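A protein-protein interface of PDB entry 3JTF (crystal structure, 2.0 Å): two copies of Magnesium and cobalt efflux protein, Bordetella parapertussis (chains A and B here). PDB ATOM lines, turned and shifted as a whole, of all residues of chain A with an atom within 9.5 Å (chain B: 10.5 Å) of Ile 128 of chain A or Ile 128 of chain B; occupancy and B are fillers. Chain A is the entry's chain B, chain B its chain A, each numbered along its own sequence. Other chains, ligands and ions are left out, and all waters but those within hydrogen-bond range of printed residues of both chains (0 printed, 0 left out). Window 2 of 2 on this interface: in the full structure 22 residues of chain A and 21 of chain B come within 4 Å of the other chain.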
ATOM      1  N   ARG A   5      -5.676 -29.488   2.357  1.00  0.00           N
ATOM      2  CA  ARG A   5      -5.753 -28.680   3.586  1.00  0.00           C
ATOM      3  C   ARG A   5      -7.170 -28.198   3.879  1.00  0.00           C
ATOM      4  O   ARG A   5      -8.004 -28.100   2.955  1.00  0.00           O
ATOM      5  CB  ARG A   5      -4.884 -27.429   3.478  1.00  0.00           C
ATOM      6  CG  ARG A   5      -3.470 -27.716   3.126  1.00  0.00           C
ATOM      7  CD  ARG A   5      -2.563 -26.660   3.640  1.00  0.00           C
ATOM      8  NE  ARG A   5      -1.206 -27.194   3.690  1.00  0.00           N
ATOM      9  CZ  ARG A   5      -0.561 -27.548   4.797  1.00  0.00           C
ATOM     10  NH1 ARG A   5      -1.134 -27.439   6.001  1.00  0.00           N
ATOM     11  NH2 ARG A   5       0.672 -28.019   4.693  1.00  0.00           N
ATOM     12  N   ASN A  88      -9.379 -25.523  -1.774  1.00  0.00           N
ATOM     13  CA  ASN A  88      -9.588 -25.379  -3.218  1.00  0.00           C
ATOM     14  C   ASN A  88     -11.066 -24.996  -3.485  1.00  0.00           C
ATOM     15  O   ASN A  88     -11.344 -24.157  -4.351  1.00  0.00           O
ATOM     16  CB  ASN A  88      -9.165 -26.625  -4.024  1.00  0.00           C
ATOM     17  CG  ASN A  88      -7.644 -26.952  -3.910  1.00  0.00           C
ATOM     18  OD1 ASN A  88      -6.796 -26.072  -3.651  1.00  0.00           O
ATOM     19  ND2 ASN A  88      -7.307 -28.233  -4.114  1.00  0.00           N
ATOM     20  N   LEU A  91     -11.721 -21.319  -2.221  1.00  0.00           N
ATOM     21  CA  LEU A  91     -11.188 -20.371  -3.190  1.00  0.00           C
ATOM     22  C   LEU A  91     -12.209 -20.063  -4.316  1.00  0.00           C
ATOM     23  O   LEU A  91     -12.422 -18.917  -4.652  1.00  0.00           O
ATOM     24  CB  LEU A  91      -9.896 -20.882  -3.803  1.00  0.00           C
ATOM     25  CG  LEU A  91      -9.285 -19.877  -4.791  1.00  0.00           C
ATOM     26  CD1 LEU A  91      -9.164 -18.456  -4.222  1.00  0.00           C
ATOM     27  CD2 LEU A  91      -7.892 -20.418  -5.264  1.00  0.00           C
ATOM     28  N   ARG A  95     -13.976 -16.504  -4.945  1.00  0.00           N
ATOM     29  CA  ARG A  95     -13.778 -15.852  -6.245  1.00  0.00           C
ATOM     30  C   ARG A  95     -15.119 -15.473  -6.894  1.00  0.00           C
ATOM     31  O   ARG A  95     -15.210 -14.452  -7.563  1.00  0.00           O
ATOM     32  CB  ARG A  95     -12.978 -16.739  -7.213  1.00  0.00           C
ATOM     33  CG  ARG A  95     -11.437 -16.666  -7.071  1.00  0.00           C
ATOM     34  CD  ARG A  95     -10.763 -17.676  -8.041  1.00  0.00           C
ATOM     35  NE  ARG A  95      -9.285 -17.701  -8.005  1.00  0.00           N
ATOM     36  CZ  ARG A  95      -8.568 -18.644  -8.595  1.00  0.00           C
ATOM     37  NH1 ARG A  95      -9.198 -19.605  -9.248  1.00  0.00           N
ATOM     38  NH2 ARG A  95      -7.232 -18.633  -8.567  1.00  0.00           N
ATOM     39  N   VAL A 120      -6.379 -17.898   1.903  1.00  0.00           N
ATOM     40  CA  VAL A 120      -6.507 -19.114   1.108  1.00  0.00           C
ATOM     41  C   VAL A 120      -5.440 -19.125  -0.012  1.00  0.00           C
ATOM     42  O   VAL A 120      -4.752 -20.118  -0.201  1.00  0.00           O
ATOM     43  CB  VAL A 120      -7.938 -19.208   0.520  1.00  0.00           C
ATOM     44  CG1 VAL A 120      -8.081 -20.416  -0.412  1.00  0.00           C
ATOM     45  CG2 VAL A 120      -9.003 -19.244   1.663  1.00  0.00           C
ATOM     46  N   LEU A 121      -5.312 -18.010  -0.732  1.00  0.00           N
ATOM     47  CA  LEU A 121      -4.400 -17.905  -1.874  1.00  0.00           C
ATOM     48  C   LEU A 121      -2.968 -18.100  -1.412  1.00  0.00           C
ATOM     49  O   LEU A 121      -2.225 -18.848  -2.010  1.00  0.00           O
ATOM     50  CB  LEU A 121      -4.536 -16.551  -2.552  1.00  0.00           C
ATOM     51  CG  LEU A 121      -5.748 -16.373  -3.453  1.00  0.00           C
ATOM     52  CD1 LEU A 121      -5.898 -14.863  -3.794  1.00  0.00           C
ATOM     53  CD2 LEU A 121      -5.580 -17.230  -4.675  1.00  0.00           C
ATOM     54  N   GLU A 122      -2.615 -17.463  -0.304  1.00  0.00           N
ATOM     55  CA  GLU A 122      -1.269 -17.587   0.238  1.00  0.00           C
ATOM     56  C   GLU A 122      -0.909 -19.023   0.607  1.00  0.00           C
ATOM     57  O   GLU A 122       0.169 -19.478   0.295  1.00  0.00           O
ATOM     58  CB  GLU A 122      -1.125 -16.699   1.459  1.00  0.00           C
ATOM     59  CG  GLU A 122      -1.074 -15.244   1.077  1.00  0.00           C
ATOM     60  CD  GLU A 122      -0.623 -14.361   2.199  1.00  0.00           C
ATOM     61  OE1 GLU A 122      -1.087 -14.590   3.340  1.00  0.00           O
ATOM     62  OE2 GLU A 122       0.196 -13.440   1.928  1.00  0.00           O
ATOM     63  N   GLN A 123      -1.824 -19.736   1.257  1.00  0.00           N
ATOM     64  CA  GLN A 123      -1.529 -21.094   1.652  1.00  0.00           C
ATOM     65  C   GLN A 123      -1.413 -21.997   0.451  1.00  0.00           C
ATOM     66  O   GLN A 123      -0.481 -22.808   0.403  1.00  0.00           O
ATOM     67  CB  GLN A 123      -2.592 -21.642   2.574  1.00  0.00           C
ATOM     68  CG  GLN A 123      -2.383 -23.076   2.947  1.00  0.00           C
ATOM     69  CD  GLN A 123      -1.150 -23.256   3.799  1.00  0.00           C
ATOM     70  OE1 GLN A 123      -0.895 -22.467   4.696  1.00  0.00           O
ATOM     71  NE2 GLN A 123      -0.375 -24.270   3.504  1.00  0.00           N
ATOM     72  N   ILE A 124      -2.354 -21.873  -0.500  1.00  0.00           N
ATOM     73  CA  ILE A 124      -2.318 -22.655  -1.730  1.00  0.00           C
ATOM     74  C   ILE A 124      -0.987 -22.429  -2.470  1.00  0.00           C
ATOM     75  O   ILE A 124      -0.348 -23.390  -2.856  1.00  0.00           O
ATOM     76  CB  ILE A 124      -3.532 -22.404  -2.679  1.00  0.00           C
ATOM     77  CG1 ILE A 124      -4.844 -22.863  -2.025  1.00  0.00           C
ATOM     78  CG2 ILE A 124      -3.316 -23.115  -4.061  1.00  0.00           C
ATOM     79  CD1 ILE A 124      -6.128 -22.553  -2.828  1.00  0.00           C
ATOM     80  N   VAL A 125      -0.571 -21.174  -2.662  1.00  0.00           N
ATOM     81  CA  VAL A 125       0.728 -20.903  -3.297  1.00  0.00           C
ATOM     82  C   VAL A 125       1.908 -21.392  -2.450  1.00  0.00           C
ATOM     83  O   VAL A 125       2.848 -21.943  -2.987  1.00  0.00           O
ATOM     84  CB  VAL A 125       0.931 -19.410  -3.573  1.00  0.00           C
ATOM     85  CG1 VAL A 125       2.369 -19.115  -3.930  1.00  0.00           C
ATOM     86  CG2 VAL A 125      -0.015 -18.972  -4.683  1.00  0.00           C
ATOM     87  N   GLY A 126       1.861 -21.179  -1.139  1.00  0.00           N
ATOM     88  CA  GLY A 126       2.847 -21.773  -0.218  1.00  0.00           C
ATOM     89  C   GLY A 126       3.021 -23.294  -0.307  1.00  0.00           C
ATOM     90  O   GLY A 126       4.102 -23.818   0.006  1.00  0.00           O
ATOM     91  N   ASP A 127       1.973 -24.010  -0.733  1.00  0.00           N
ATOM     92  CA  ASP A 127       2.052 -25.470  -0.916  1.00  0.00           C
ATOM     93  C   ASP A 127       2.471 -25.918  -2.319  1.00  0.00           C
ATOM     94  O   ASP A 127       2.469 -27.115  -2.594  1.00  0.00           O
ATOM     95  CB  ASP A 127       0.707 -26.121  -0.581  1.00  0.00           C
ATOM     96  CG  ASP A 127       0.425 -26.141   0.894  1.00  0.00           C
ATOM     97  OD1 ASP A 127       1.387 -25.998   1.692  1.00  0.00           O
ATOM     98  OD2 ASP A 127      -0.761 -26.306   1.259  1.00  0.00           O
ATOM     99  N   ILE A 128       2.821 -24.972  -3.196  1.00  0.00           N
ATOM    100  CA  ILE A 128       3.239 -25.287  -4.572  1.00  0.00           C
ATOM    101  C   ILE A 128       4.659 -24.788  -4.843  1.00  0.00           C
ATOM    102  O   ILE A 128       5.565 -24.983  -4.022  1.00  0.00           O
ATOM    103  CB  ILE A 128       2.244 -24.737  -5.662  1.00  0.00           C
ATOM    104  CG1 ILE A 128       2.507 -23.280  -6.046  1.00  0.00           C
ATOM    105  CG2 ILE A 128       0.805 -24.877  -5.218  1.00  0.00           C
ATOM    106  CD1 ILE A 128       1.945 -22.949  -7.424  1.00  0.00           C
ATOM    107  N   ARG B   5       6.229 -15.541 -16.884  1.00  0.00           N
ATOM    108  CA  ARG B   5       5.230 -14.457 -16.871  1.00  0.00           C
ATOM    109  C   ARG B   5       5.692 -13.151 -16.217  1.00  0.00           C
ATOM    110  O   ARG B   5       6.461 -13.155 -15.260  1.00  0.00           O
ATOM    111  CB  ARG B   5       3.952 -14.923 -16.176  1.00  0.00           C
ATOM    112  CG  ARG B   5       3.128 -15.862 -17.017  1.00  0.00           C
ATOM    113  CD  ARG B   5       2.184 -16.615 -16.145  1.00  0.00           C
ATOM    114  NE  ARG B   5       0.969 -16.964 -16.868  1.00  0.00           N
ATOM    115  CZ  ARG B   5       0.861 -17.947 -17.767  1.00  0.00           C
ATOM    116  NH1 ARG B   5      -0.315 -18.169 -18.346  1.00  0.00           N
ATOM    117  NH2 ARG B   5       1.905 -18.705 -18.103  1.00  0.00           N
ATOM    118  N   ASN B  88       7.417 -14.015 -10.214  1.00  0.00           N
ATOM    119  CA  ASN B  88       8.030 -14.629  -9.042  1.00  0.00           C
ATOM    120  C   ASN B  88       8.856 -13.598  -8.245  1.00  0.00           C
ATOM    121  O   ASN B  88       8.798 -13.544  -7.008  1.00  0.00           O
ATOM    122  CB  ASN B  88       8.847 -15.869  -9.447  1.00  0.00           C
ATOM    123  CG  ASN B  88       7.950 -17.133  -9.683  1.00  0.00           C
ATOM    124  OD1 ASN B  88       6.706 -17.083  -9.586  1.00  0.00           O
ATOM    125  ND2 ASN B  88       8.593 -18.261  -9.982  1.00  0.00           N
ATOM    126  N   LEU B  91       6.284 -11.371  -6.320  1.00  0.00           N
ATOM    127  CA  LEU B  91       5.680 -12.064  -5.176  1.00  0.00           C
ATOM    128  C   LEU B  91       6.618 -12.009  -3.949  1.00  0.00           C
ATOM    129  O   LEU B  91       6.207 -11.657  -2.845  1.00  0.00           O
ATOM    130  CB  LEU B  91       5.389 -13.532  -5.533  1.00  0.00           C
ATOM    131  CG  LEU B  91       4.261 -14.218  -4.731  1.00  0.00           C
ATOM    132  CD1 LEU B  91       4.573 -15.684  -4.498  1.00  0.00           C
ATOM    133  CD2 LEU B  91       3.972 -13.534  -3.424  1.00  0.00           C
ATOM    134  N   VAL B 120      -1.181 -11.422  -8.301  1.00  0.00           N
ATOM    135  CA  VAL B 120      -0.019 -12.286  -8.440  1.00  0.00           C
ATOM    136  C   VAL B 120      -0.314 -13.723  -7.968  1.00  0.00           C
ATOM    137  O   VAL B 120      -0.058 -14.690  -8.679  1.00  0.00           O
ATOM    138  CB  VAL B 120       1.184 -11.692  -7.652  1.00  0.00           C
ATOM    139  CG1 VAL B 120       2.377 -12.676  -7.635  1.00  0.00           C
ATOM    140  CG2 VAL B 120       1.592 -10.329  -8.230  1.00  0.00           C
ATOM    141  N   LEU B 121      -0.880 -13.854  -6.776  1.00  0.00           N
ATOM    142  CA  LEU B 121      -1.273 -15.153  -6.238  1.00  0.00           C
ATOM    143  C   LEU B 121      -2.320 -15.905  -7.103  1.00  0.00           C
ATOM    144  O   LEU B 121      -2.210 -17.111  -7.364  1.00  0.00           O
ATOM    145  CB  LEU B 121      -1.793 -14.951  -4.799  1.00  0.00           C
ATOM    146  CG  LEU B 121      -0.801 -14.446  -3.749  1.00  0.00           C
ATOM    147  CD1 LEU B 121      -1.489 -14.067  -2.411  1.00  0.00           C
ATOM    148  CD2 LEU B 121       0.258 -15.454  -3.521  1.00  0.00           C
ATOM    149  N   GLU B 122      -3.333 -15.174  -7.555  1.00  0.00           N
ATOM    150  CA  GLU B 122      -4.358 -15.750  -8.428  1.00  0.00           C
ATOM    151  C   GLU B 122      -3.741 -16.337  -9.671  1.00  0.00           C
ATOM    152  O   GLU B 122      -4.072 -17.450 -10.027  1.00  0.00           O
ATOM    153  CB  GLU B 122      -5.416 -14.719  -8.785  1.00  0.00           C
ATOM    154  CG  GLU B 122      -6.368 -14.520  -7.643  1.00  0.00           C
ATOM    155  CD  GLU B 122      -7.447 -13.476  -7.901  1.00  0.00           C
ATOM    156  OE1 GLU B 122      -7.222 -12.589  -8.749  1.00  0.00           O
ATOM    157  OE2 GLU B 122      -8.511 -13.526  -7.231  1.00  0.00           O
ATOM    158  N   GLN B 123      -2.820 -15.597 -10.305  1.00  0.00           N
ATOM    159  CA  GLN B 123      -2.111 -16.114 -11.481  1.00  0.00           C
ATOM    160  C   GLN B 123      -1.325 -17.347 -11.155  1.00  0.00           C
ATOM    161  O   GLN B 123      -1.383 -18.335 -11.889  1.00  0.00           O
ATOM    162  CB  GLN B 123      -1.156 -15.075 -12.100  1.00  0.00           C
ATOM    163  CG  GLN B 123      -0.409 -15.554 -13.392  1.00  0.00           C
ATOM    164  CD  GLN B 123      -1.375 -15.939 -14.513  1.00  0.00           C
ATOM    165  OE1 GLN B 123      -1.118 -16.880 -15.259  1.00  0.00           O
ATOM    166  NE2 GLN B 123      -2.512 -15.242 -14.602  1.00  0.00           N
ATOM    167  N   ILE B 124      -0.604 -17.333 -10.046  1.00  0.00           N
ATOM    168  CA  ILE B 124       0.188 -18.534  -9.694  1.00  0.00           C
ATOM    169  C   ILE B 124      -0.682 -19.744  -9.412  1.00  0.00           C
ATOM    170  O   ILE B 124      -0.346 -20.868  -9.788  1.00  0.00           O
ATOM    171  CB  ILE B 124       1.120 -18.270  -8.500  1.00  0.00           C
ATOM    172  CG1 ILE B 124       2.096 -17.149  -8.864  1.00  0.00           C
ATOM    173  CG2 ILE B 124       1.820 -19.534  -8.116  1.00  0.00           C
ATOM    174  CD1 ILE B 124       2.921 -16.626  -7.710  1.00  0.00           C
ATOM    175  N   VAL B 125      -1.819 -19.536  -8.749  1.00  0.00           N
ATOM    176  CA  VAL B 125      -2.754 -20.645  -8.531  1.00  0.00           C
ATOM    177  C   VAL B 125      -3.355 -21.158  -9.835  1.00  0.00           C
ATOM    178  O   VAL B 125      -3.521 -22.358  -9.999  1.00  0.00           O
ATOM    179  CB  VAL B 125      -3.882 -20.296  -7.529  1.00  0.00           C
ATOM    180  CG1 VAL B 125      -4.898 -21.427  -7.456  1.00  0.00           C
ATOM    181  CG2 VAL B 125      -3.277 -19.983  -6.175  1.00  0.00           C
ATOM    182  N   GLY B 126      -3.685 -20.267 -10.762  1.00  0.00           N
ATOM    183  CA  GLY B 126      -4.186 -20.712 -12.073  1.00  0.00           C
ATOM    184  C   GLY B 126      -3.146 -21.464 -12.929  1.00  0.00           C
ATOM    185  O   GLY B 126      -3.513 -22.214 -13.840  1.00  0.00           O
ATOM    186  N   ASP B 127      -1.852 -21.257 -12.658  1.00  0.00           N
ATOM    187  CA  ASP B 127      -0.777 -21.952 -13.400  1.00  0.00           C
ATOM    188  C   ASP B 127      -0.371 -23.301 -12.769  1.00  0.00           C
ATOM    189  O   ASP B 127       0.613 -23.895 -13.189  1.00  0.00           O
ATOM    190  CB  ASP B 127       0.457 -21.042 -13.549  1.00  0.00           C
ATOM    191  CG  ASP B 127       0.198 -19.844 -14.452  1.00  0.00           C
ATOM    192  OD1 ASP B 127      -0.756 -19.917 -15.264  1.00  0.00           O
ATOM    193  OD2 ASP B 127       0.933 -18.826 -14.351  1.00  0.00           O
ATOM    194  N   ILE B 128      -1.127 -23.785 -11.779  1.00  0.00           N
ATOM    195  CA  ILE B 128      -0.862 -25.090 -11.156  1.00  0.00           C
ATOM    196  C   ILE B 128      -1.221 -26.233 -12.117  1.00  0.00           C
ATOM    197  O   ILE B 128      -2.312 -26.248 -12.690  1.00  0.00           O
ATOM    198  CB  ILE B 128      -1.641 -25.269  -9.811  1.00  0.00           C
ATOM    199  CG1 ILE B 128      -1.085 -24.319  -8.745  1.00  0.00           C
ATOM    200  CG2 ILE B 128      -1.572 -26.730  -9.308  1.00  0.00           C
ATOM    201  CD1 ILE B 128      -1.763 -24.464  -7.382  1.00  0.00           C
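Printed residues of chain B within 4 Å of Arg 95 of chain A: Glu 122 and Val 125. Printed residues of chain B within 4 Å of Leu 121 of chain A: Leu 121 (3.9 Å), Glu 122 (3.9 Å) and Val 125 (3.9 Å). Of the printed residues of chain B, Glu 122 of chain A touches Leu 121 (3.7 Å). Gly 126 of chain A touches none of the printed residues of chain B. No residue of chain B comes within 4 Å of Asp 127 of chain A. Ile 128 of chain A touches just these residues of chain B: Ile 124 and Ile 128. Asn 88 of chain B touches none of the printed residues of chain A. Leu 91 of chain B touches none of the printed residues of chain A. Of the printed residues of chain A, Ile 124 of chain B touches Val 125 and Ile 128. No residue of chain A comes within 4 Å of Gly 126 of chain B. Of the printed residues of chain A, Ile 128 of chain B touches Ile 124 (3.9 Å) and Ile 128 (3.4 Å). The nearest printed residue of chain A that does not touch Glu 122 of chain B is Val 125 of chain A (5.8 Å).
Of the 12 printed residues of chain B, 5 touch a printed residue of chain A. Printed residues of chain B that touch a printed residue of chain A: Leu 121, Glu 122, Ile 124, Val 125 and Ile 128. Hydrophobic or aromatic side chains of chain B within 4 Å of the printed part of chain A: Leu 121, Ile 124, Val 125 and Ile 128.
Leu 91 of chain A touches Val 125 of chain B, but with the chains exchanged Val 125 of chain A does not touch Leu 91 of chain B (4.1 Å). Ile 124 of chain A touches Ile 128 of chain B, and with the chains exchanged Ile 128 of chain A touches Ile 124 of chain B. Val 125 of chain B touches its own counterpart, Val 125 of chain A. Ile 128 of chain B touches its own counterpart, Ile 128 of chain A. 12 positions are printed for both chains. Of the 14 pairs that touch across the chains among the printed residues, 11 have their exchanged pair printed and touching as well.
Among the printed residues, merely in contact across the chains: Ile 128 of chain A with Ile 128 of chain B (3.4 Å), Ile 128 of chain A with Ile 124 of chain B (3.5 Å), Arg 95 of chain A with Glu 122 of chain B (3.7 Å), Glu 122 of chain A with Leu 121 of chain B (3.7 Å), Val 125 of chain A with Leu 121 of chain B (3.7 Å), Val 125 of chain A with Val 125 of chain B (3.7 Å), Ile 124 of chain A with Val 125 of chain B (3.8 Å), Arg 95 of chain A with Val 125 of chain B (3.8 Å), Leu 91 of chain A with Val 125 of chain B (3.8 Å), Leu 121 of chain A with Val 125 of chain B (3.9 Å), Leu 121 of chain A with Leu 121 of chain B (3.9 Å), Leu 121 of chain A with Glu 122 of chain B (3.9 Å), Ile 124 of chain A with Ile 128 of chain B (3.9 Å) and Val 125 of chain A with Ile 124 of chain B (3.9 Å).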
